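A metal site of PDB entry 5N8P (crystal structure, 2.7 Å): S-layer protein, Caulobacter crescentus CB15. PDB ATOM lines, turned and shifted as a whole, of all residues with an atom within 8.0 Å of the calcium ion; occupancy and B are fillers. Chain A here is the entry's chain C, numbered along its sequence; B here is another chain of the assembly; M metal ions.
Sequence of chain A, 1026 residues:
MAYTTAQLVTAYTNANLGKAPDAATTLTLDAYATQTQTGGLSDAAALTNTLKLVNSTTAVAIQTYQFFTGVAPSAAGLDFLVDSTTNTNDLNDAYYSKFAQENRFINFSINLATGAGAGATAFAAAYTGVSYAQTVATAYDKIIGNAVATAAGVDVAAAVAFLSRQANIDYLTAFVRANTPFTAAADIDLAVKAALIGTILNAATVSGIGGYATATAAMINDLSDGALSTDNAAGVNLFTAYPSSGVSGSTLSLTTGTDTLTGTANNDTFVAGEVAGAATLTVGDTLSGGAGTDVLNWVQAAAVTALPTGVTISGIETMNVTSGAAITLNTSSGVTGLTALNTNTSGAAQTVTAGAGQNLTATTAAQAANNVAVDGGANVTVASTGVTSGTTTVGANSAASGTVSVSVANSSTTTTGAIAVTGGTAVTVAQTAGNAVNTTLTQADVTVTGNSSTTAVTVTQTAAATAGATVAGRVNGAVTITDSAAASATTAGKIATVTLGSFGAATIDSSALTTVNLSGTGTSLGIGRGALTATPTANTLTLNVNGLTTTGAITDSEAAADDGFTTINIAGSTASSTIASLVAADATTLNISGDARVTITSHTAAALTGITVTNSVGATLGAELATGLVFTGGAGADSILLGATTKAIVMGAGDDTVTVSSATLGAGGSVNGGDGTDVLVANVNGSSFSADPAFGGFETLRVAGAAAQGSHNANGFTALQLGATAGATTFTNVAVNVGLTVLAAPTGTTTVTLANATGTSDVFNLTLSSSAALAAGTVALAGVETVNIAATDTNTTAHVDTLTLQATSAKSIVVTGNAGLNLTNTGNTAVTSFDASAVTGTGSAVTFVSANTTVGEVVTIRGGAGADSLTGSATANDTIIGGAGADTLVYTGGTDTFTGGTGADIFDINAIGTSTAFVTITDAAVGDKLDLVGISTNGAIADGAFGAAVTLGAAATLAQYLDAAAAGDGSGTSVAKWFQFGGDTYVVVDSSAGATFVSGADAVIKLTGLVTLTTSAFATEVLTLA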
ATOM      1  N   SER A 253     -14.447  -2.460  11.920  1.00  0.00           N
ATOM      2  CA  SER A 253     -15.096  -2.557  13.212  1.00  0.00           C
ATOM      3  C   SER A 253     -14.587  -1.638  14.303  1.00  0.00           C
ATOM      4  O   SER A 253     -13.425  -1.731  14.646  1.00  0.00           O
ATOM      5  CB  SER A 253     -14.995  -3.985  13.739  1.00  0.00           C
ATOM      6  OG  SER A 253     -16.038  -4.758  13.242  1.00  0.00           O
ATOM      7  N   LEU A 254     -15.445  -0.818  14.874  1.00  0.00           N
ATOM      8  CA  LEU A 254     -15.115   0.015  16.037  1.00  0.00           C
ATOM      9  C   LEU A 254     -15.006  -0.818  17.300  1.00  0.00           C
ATOM     10  O   LEU A 254     -15.702  -1.803  17.413  1.00  0.00           O
ATOM     11  CB  LEU A 254     -16.120   1.146  16.247  1.00  0.00           C
ATOM     12  CG  LEU A 254     -15.924   2.450  15.452  1.00  0.00           C
ATOM     13  CD1 LEU A 254     -16.317   2.297  14.014  1.00  0.00           C
ATOM     14  CD2 LEU A 254     -16.726   3.586  16.064  1.00  0.00           C
ATOM     15  N   THR A 255     -14.134  -0.418  18.226  1.00  0.00           N
ATOM     16  CA  THR A 255     -13.924  -1.118  19.536  1.00  0.00           C
ATOM     17  C   THR A 255     -14.295  -0.208  20.706  1.00  0.00           C
ATOM     18  O   THR A 255     -14.565   0.979  20.489  1.00  0.00           O
ATOM     19  CB  THR A 255     -12.476  -1.523  19.755  1.00  0.00           C
ATOM     20  OG1 THR A 255     -11.726  -0.361  20.143  1.00  0.00           O
ATOM     21  CG2 THR A 255     -11.904  -2.152  18.482  1.00  0.00           C
ATOM     22  N   THR A 256     -14.252  -0.709  21.938  1.00  0.00           N
ATOM     23  CA  THR A 256     -14.548   0.170  23.058  1.00  0.00           C
ATOM     24  C   THR A 256     -13.409   1.205  23.303  1.00  0.00           C
ATOM     25  O   THR A 256     -13.511   1.990  24.251  1.00  0.00           O
ATOM     26  CB  THR A 256     -14.781  -0.605  24.375  1.00  0.00           C
ATOM     27  OG1 THR A 256     -13.588  -1.331  24.716  1.00  0.00           O
ATOM     28  CG2 THR A 256     -15.936  -1.487  24.254  1.00  0.00           C
ATOM     29  N   GLY A 257     -12.396   1.210  22.435  1.00  0.00           N
ATOM     30  CA  GLY A 257     -11.294   2.186  22.535  1.00  0.00           C
ATOM     31  C   GLY A 257     -11.388   3.473  21.696  1.00  0.00           C
ATOM     32  O   GLY A 257     -12.477   3.987  21.405  1.00  0.00           O
ATOM     33  N   THR A 258     -10.226   4.012  21.337  1.00  0.00           N
ATOM     34  CA  THR A 258     -10.174   5.103  20.383  1.00  0.00           C
ATOM     35  C   THR A 258      -9.717   4.563  19.034  1.00  0.00           C
ATOM     36  O   THR A 258      -8.591   4.101  18.894  1.00  0.00           O
ATOM     37  CB  THR A 258      -9.268   6.234  20.891  1.00  0.00           C
ATOM     38  OG1 THR A 258      -9.880   6.791  22.050  1.00  0.00           O
ATOM     39  CG2 THR A 258      -9.093   7.302  19.866  1.00  0.00           C
ATOM     40  N   ASP A 259     -10.594   4.639  18.049  1.00  0.00           N
ATOM     41  CA  ASP A 259     -10.343   4.021  16.761  1.00  0.00           C
ATOM     42  C   ASP A 259      -9.964   5.044  15.721  1.00  0.00           C
ATOM     43  O   ASP A 259     -10.485   6.169  15.713  1.00  0.00           O
ATOM     44  CB  ASP A 259     -11.575   3.250  16.311  1.00  0.00           C
ATOM     45  CG  ASP A 259     -12.040   2.271  17.386  1.00  0.00           C
ATOM     46  OD1 ASP A 259     -11.400   1.210  17.584  1.00  0.00           O
ATOM     47  OD2 ASP A 259     -13.051   2.569  18.059  1.00  0.00           O
ATOM     48  N   THR A 260      -9.009   4.648  14.881  1.00  0.00           N
ATOM     49  CA  THR A 260      -8.607   5.491  13.763  1.00  0.00           C
ATOM     50  C   THR A 260      -8.753   4.697  12.461  1.00  0.00           C
ATOM     51  O   THR A 260      -7.846   3.981  12.019  1.00  0.00           O
ATOM     52  CB  THR A 260      -7.191   6.071  13.976  1.00  0.00           C
ATOM     53  OG1 THR A 260      -7.092   6.594  15.316  1.00  0.00           O
ATOM     54  CG2 THR A 260      -6.924   7.209  12.943  1.00  0.00           C
ATOM     55  N   LEU A 261      -9.941   4.813  11.844  1.00  0.00           N
ATOM     56  CA  LEU A 261     -10.302   3.950  10.740  1.00  0.00           C
ATOM     57  C   LEU A 261     -10.436   4.732   9.444  1.00  0.00           C
ATOM     58  O   LEU A 261     -10.998   5.837   9.416  1.00  0.00           O
ATOM     59  CB  LEU A 261     -11.599   3.217  11.058  1.00  0.00           C
ATOM     60  CG  LEU A 261     -11.621   2.347  12.351  1.00  0.00           C
ATOM     61  CD1 LEU A 261     -12.954   1.692  12.548  1.00  0.00           C
ATOM     62  CD2 LEU A 261     -10.497   1.318  12.407  1.00  0.00           C
ATOM     63  N   VAL A 271     -18.692  -0.527  11.201  1.00  0.00           N
ATOM     64  CA  VAL A 271     -19.604  -1.086  12.212  1.00  0.00           C
ATOM     65  C   VAL A 271     -19.349  -0.572  13.618  1.00  0.00           C
ATOM     66  O   VAL A 271     -18.285  -0.741  14.144  1.00  0.00           O
ATOM     67  CB  VAL A 271     -19.645  -2.635  12.170  1.00  0.00           C
ATOM     68  CG1 VAL A 271     -20.643  -3.183  13.221  1.00  0.00           C
ATOM     69  CG2 VAL A 271     -20.045  -3.149  10.791  1.00  0.00           C
ATOM     70  N   ALA A 272     -20.344   0.063  14.184  1.00  0.00           N
ATOM     71  CA  ALA A 272     -20.226   0.612  15.525  1.00  0.00           C
ATOM     72  C   ALA A 272     -21.195   0.002  16.494  1.00  0.00           C
ATOM     73  O   ALA A 272     -22.018   0.723  17.089  1.00  0.00           O
ATOM     74  CB  ALA A 272     -20.336   2.150  15.474  1.00  0.00           C
ATOM     75  N   ALA A 279     -20.737   0.592  24.463  1.00  0.00           N
ATOM     76  CA  ALA A 279     -20.778   1.253  23.150  1.00  0.00           C
ATOM     77  C   ALA A 279     -19.418   1.223  22.462  1.00  0.00           C
ATOM     78  O   ALA A 279     -18.376   1.273  23.155  1.00  0.00           O
ATOM     79  CB  ALA A 279     -21.225   2.686  23.348  1.00  0.00           C
ATOM     80  N   THR A 280     -19.397   1.147  21.130  1.00  0.00           N
ATOM     81  CA  THR A 280     -18.080   1.253  20.422  1.00  0.00           C
ATOM     82  C   THR A 280     -17.810   2.574  19.701  1.00  0.00           C
ATOM     83  O   THR A 280     -16.697   2.807  19.248  1.00  0.00           O
ATOM     84  CB  THR A 280     -17.744   0.058  19.521  1.00  0.00           C
ATOM     85  OG1 THR A 280     -18.563   0.066  18.371  1.00  0.00           O
ATOM     86  CG2 THR A 280     -17.869  -1.238  20.283  1.00  0.00           C
ATOM     87  N   LEU A 281     -18.813   3.444  19.601  1.00  0.00           N
ATOM     88  CA  LEU A 281     -18.547   4.816  19.240  1.00  0.00           C
ATOM     89  C   LEU A 281     -18.272   5.569  20.552  1.00  0.00           C
ATOM     90  O   LEU A 281     -19.156   5.718  21.409  1.00  0.00           O
ATOM     91  CB  LEU A 281     -19.727   5.403  18.455  1.00  0.00           C
ATOM     92  CG  LEU A 281     -19.338   6.670  17.660  1.00  0.00           C
ATOM     93  CD1 LEU A 281     -18.659   6.387  16.302  1.00  0.00           C
ATOM     94  CD2 LEU A 281     -20.650   7.424  17.432  1.00  0.00           C
ATOM     95  N   THR A 282     -17.022   5.975  20.705  1.00  0.00           N
ATOM     96  CA  THR A 282     -16.480   6.442  21.984  1.00  0.00           C
ATOM     97  C   THR A 282     -15.511   7.596  21.745  1.00  0.00           C
ATOM     98  O   THR A 282     -15.130   7.882  20.615  1.00  0.00           O
ATOM     99  CB  THR A 282     -15.658   5.372  22.685  1.00  0.00           C
ATOM    100  OG1 THR A 282     -14.909   4.677  21.685  1.00  0.00           O
ATOM    101  CG2 THR A 282     -16.542   4.385  23.386  1.00  0.00           C
ATOM    102  N   VAL A 283     -15.084   8.219  22.845  1.00  0.00           N
ATOM    103  CA  VAL A 283     -14.270   9.411  22.796  1.00  0.00           C
ATOM    104  C   VAL A 283     -13.055   9.306  21.865  1.00  0.00           C
ATOM    105  O   VAL A 283     -12.343   8.293  21.903  1.00  0.00           O
ATOM    106  CB  VAL A 283     -13.993  10.027  24.206  1.00  0.00           C
ATOM    107  CG1 VAL A 283     -15.087   9.675  25.206  1.00  0.00           C
ATOM    108  CG2 VAL A 283     -12.614   9.683  24.692  1.00  0.00           C
ATOM    109  N   GLY A 284     -12.881  10.293  20.988  1.00  0.00           N
ATOM    110  CA  GLY A 284     -11.731  10.382  20.111  1.00  0.00           C
ATOM    111  C   GLY A 284     -11.766   9.575  18.817  1.00  0.00           C
ATOM    112  O   GLY A 284     -10.901   9.773  17.942  1.00  0.00           O
ATOM    113  N   ASP A 285     -12.754   8.687  18.689  1.00  0.00           N
ATOM    114  CA  ASP A 285     -12.945   7.896  17.472  1.00  0.00           C
ATOM    115  C   ASP A 285     -12.916   8.794  16.224  1.00  0.00           C
ATOM    116  O   ASP A 285     -13.688   9.752  16.116  1.00  0.00           O
ATOM    117  CB  ASP A 285     -14.302   7.164  17.503  1.00  0.00           C
ATOM    118  CG  ASP A 285     -14.319   5.919  18.373  1.00  0.00           C
ATOM    119  OD1 ASP A 285     -15.423   5.418  18.661  1.00  0.00           O
ATOM    120  OD2 ASP A 285     -13.241   5.412  18.786  1.00  0.00           O
ATOM    121  N   THR A 286     -12.004   8.509  15.296  1.00  0.00           N
ATOM    122  CA  THR A 286     -12.066   9.270  14.051  1.00  0.00           C
ATOM    123  C   THR A 286     -12.180   8.337  12.843  1.00  0.00           C
ATOM    124  O   THR A 286     -11.358   7.401  12.668  1.00  0.00           O
ATOM    125  CB  THR A 286     -10.947  10.364  13.887  1.00  0.00           C
ATOM    126  OG1 THR A 286      -9.707   9.732  13.582  1.00  0.00           O
ATOM    127  CG2 THR A 286     -10.809  11.308  15.147  1.00  0.00           C
ATOM    128  N   LEU A 287     -13.223   8.585  12.037  1.00  0.00           N
ATOM    129  CA  LEU A 287     -13.546   7.751  10.880  1.00  0.00           C
ATOM    130  C   LEU A 287     -13.466   8.542   9.590  1.00  0.00           C
ATOM    131  O   LEU A 287     -13.865   9.725   9.521  1.00  0.00           O
ATOM    132  CB  LEU A 287     -14.927   7.099  11.040  1.00  0.00           C
ATOM    133  CG  LEU A 287     -15.265   6.451  12.388  1.00  0.00           C
ATOM    134  CD1 LEU A 287     -16.736   6.057  12.430  1.00  0.00           C
ATOM    135  CD2 LEU A 287     -14.441   5.230  12.671  1.00  0.00           C
ATOM    136  N   VAL A 311     -14.946  12.892  18.606  1.00  0.00           N
ATOM    137  CA  VAL A 311     -15.407  12.089  17.478  1.00  0.00           C
ATOM    138  C   VAL A 311     -15.515  12.986  16.264  1.00  0.00           C
ATOM    139  O   VAL A 311     -16.050  14.114  16.351  1.00  0.00           O
ATOM    140  CB  VAL A 311     -16.745  11.351  17.795  1.00  0.00           C
ATOM    141  CG1 VAL A 311     -17.418  10.791  16.547  1.00  0.00           C
ATOM    142  CG2 VAL A 311     -16.521  10.257  18.820  1.00  0.00           C
ATOM    143  N   GLU B 274      -8.971   6.639  24.822  1.00  0.00           N
ATOM    144  CA  GLU B 274      -9.535   5.998  25.999  1.00  0.00           C
ATOM    145  C   GLU B 274      -9.685   4.509  25.805  1.00  0.00           C
ATOM    146  O   GLU B 274      -9.727   4.046  24.665  1.00  0.00           O
ATOM    147  CB  GLU B 274     -10.873   6.588  26.280  1.00  0.00           C
ATOM    148  CG  GLU B 274     -10.759   7.852  27.102  1.00  0.00           C
ATOM    149  CD  GLU B 274     -12.085   8.384  27.555  1.00  0.00           C
ATOM    150  OE1 GLU B 274     -13.158   7.844  27.159  1.00  0.00           O
ATOM    151  OE2 GLU B 274     -12.009   9.344  28.317  1.00  0.00           O
ATOM    152  N   VAL B 275      -9.715   3.759  26.910  1.00  0.00           N
ATOM    153  CA  VAL B 275     -10.016   2.333  26.814  1.00  0.00           C
ATOM    154  C   VAL B 275     -11.386   1.926  27.341  1.00  0.00           C
ATOM    155  O   VAL B 275     -12.199   1.423  26.580  1.00  0.00           O
ATOM    156  CB  VAL B 275      -8.822   1.403  27.127  1.00  0.00           C
ATOM    157  CG1 VAL B 275      -9.233   0.199  27.966  1.00  0.00           C
ATOM    158  CG2 VAL B 275      -8.207   0.933  25.804  1.00  0.00           C
HETATM  159 CA    CA M   1     -14.176   3.275  19.649  1.00  0.00          CA
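The backbone carbonyl oxygen (O) of Asp 259 is in hydrogen-bond range of the backbone NH (N) of Thr 286, 2.8 Å away. The side-chain hydroxyl of Thr 255 sits at hydrogen-bond distance from the backbone NH of Gly 257 (2.9 Å).
Within 4 Å of the calcium ion: Thr 255, Gly 257, Asp 259, Thr 280, Thr 282 and Asp 285.
The calcium ion is bound by the side-chain carboxylate (OD2) of Asp 259, the backbone carbonyl oxygen (O) of Thr 255, the side-chain carboxylate (OD2) of Asp 285, the backbone carbonyl oxygen (O) of Gly 257, the side-chain hydroxyl (OG1) of Thr 282, the backbone carbonyl oxygen (O) of Thr 280 and the side-chain carboxylate (OD1) of Asp 285. The calcium ion has seven donor atoms within binding distance.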
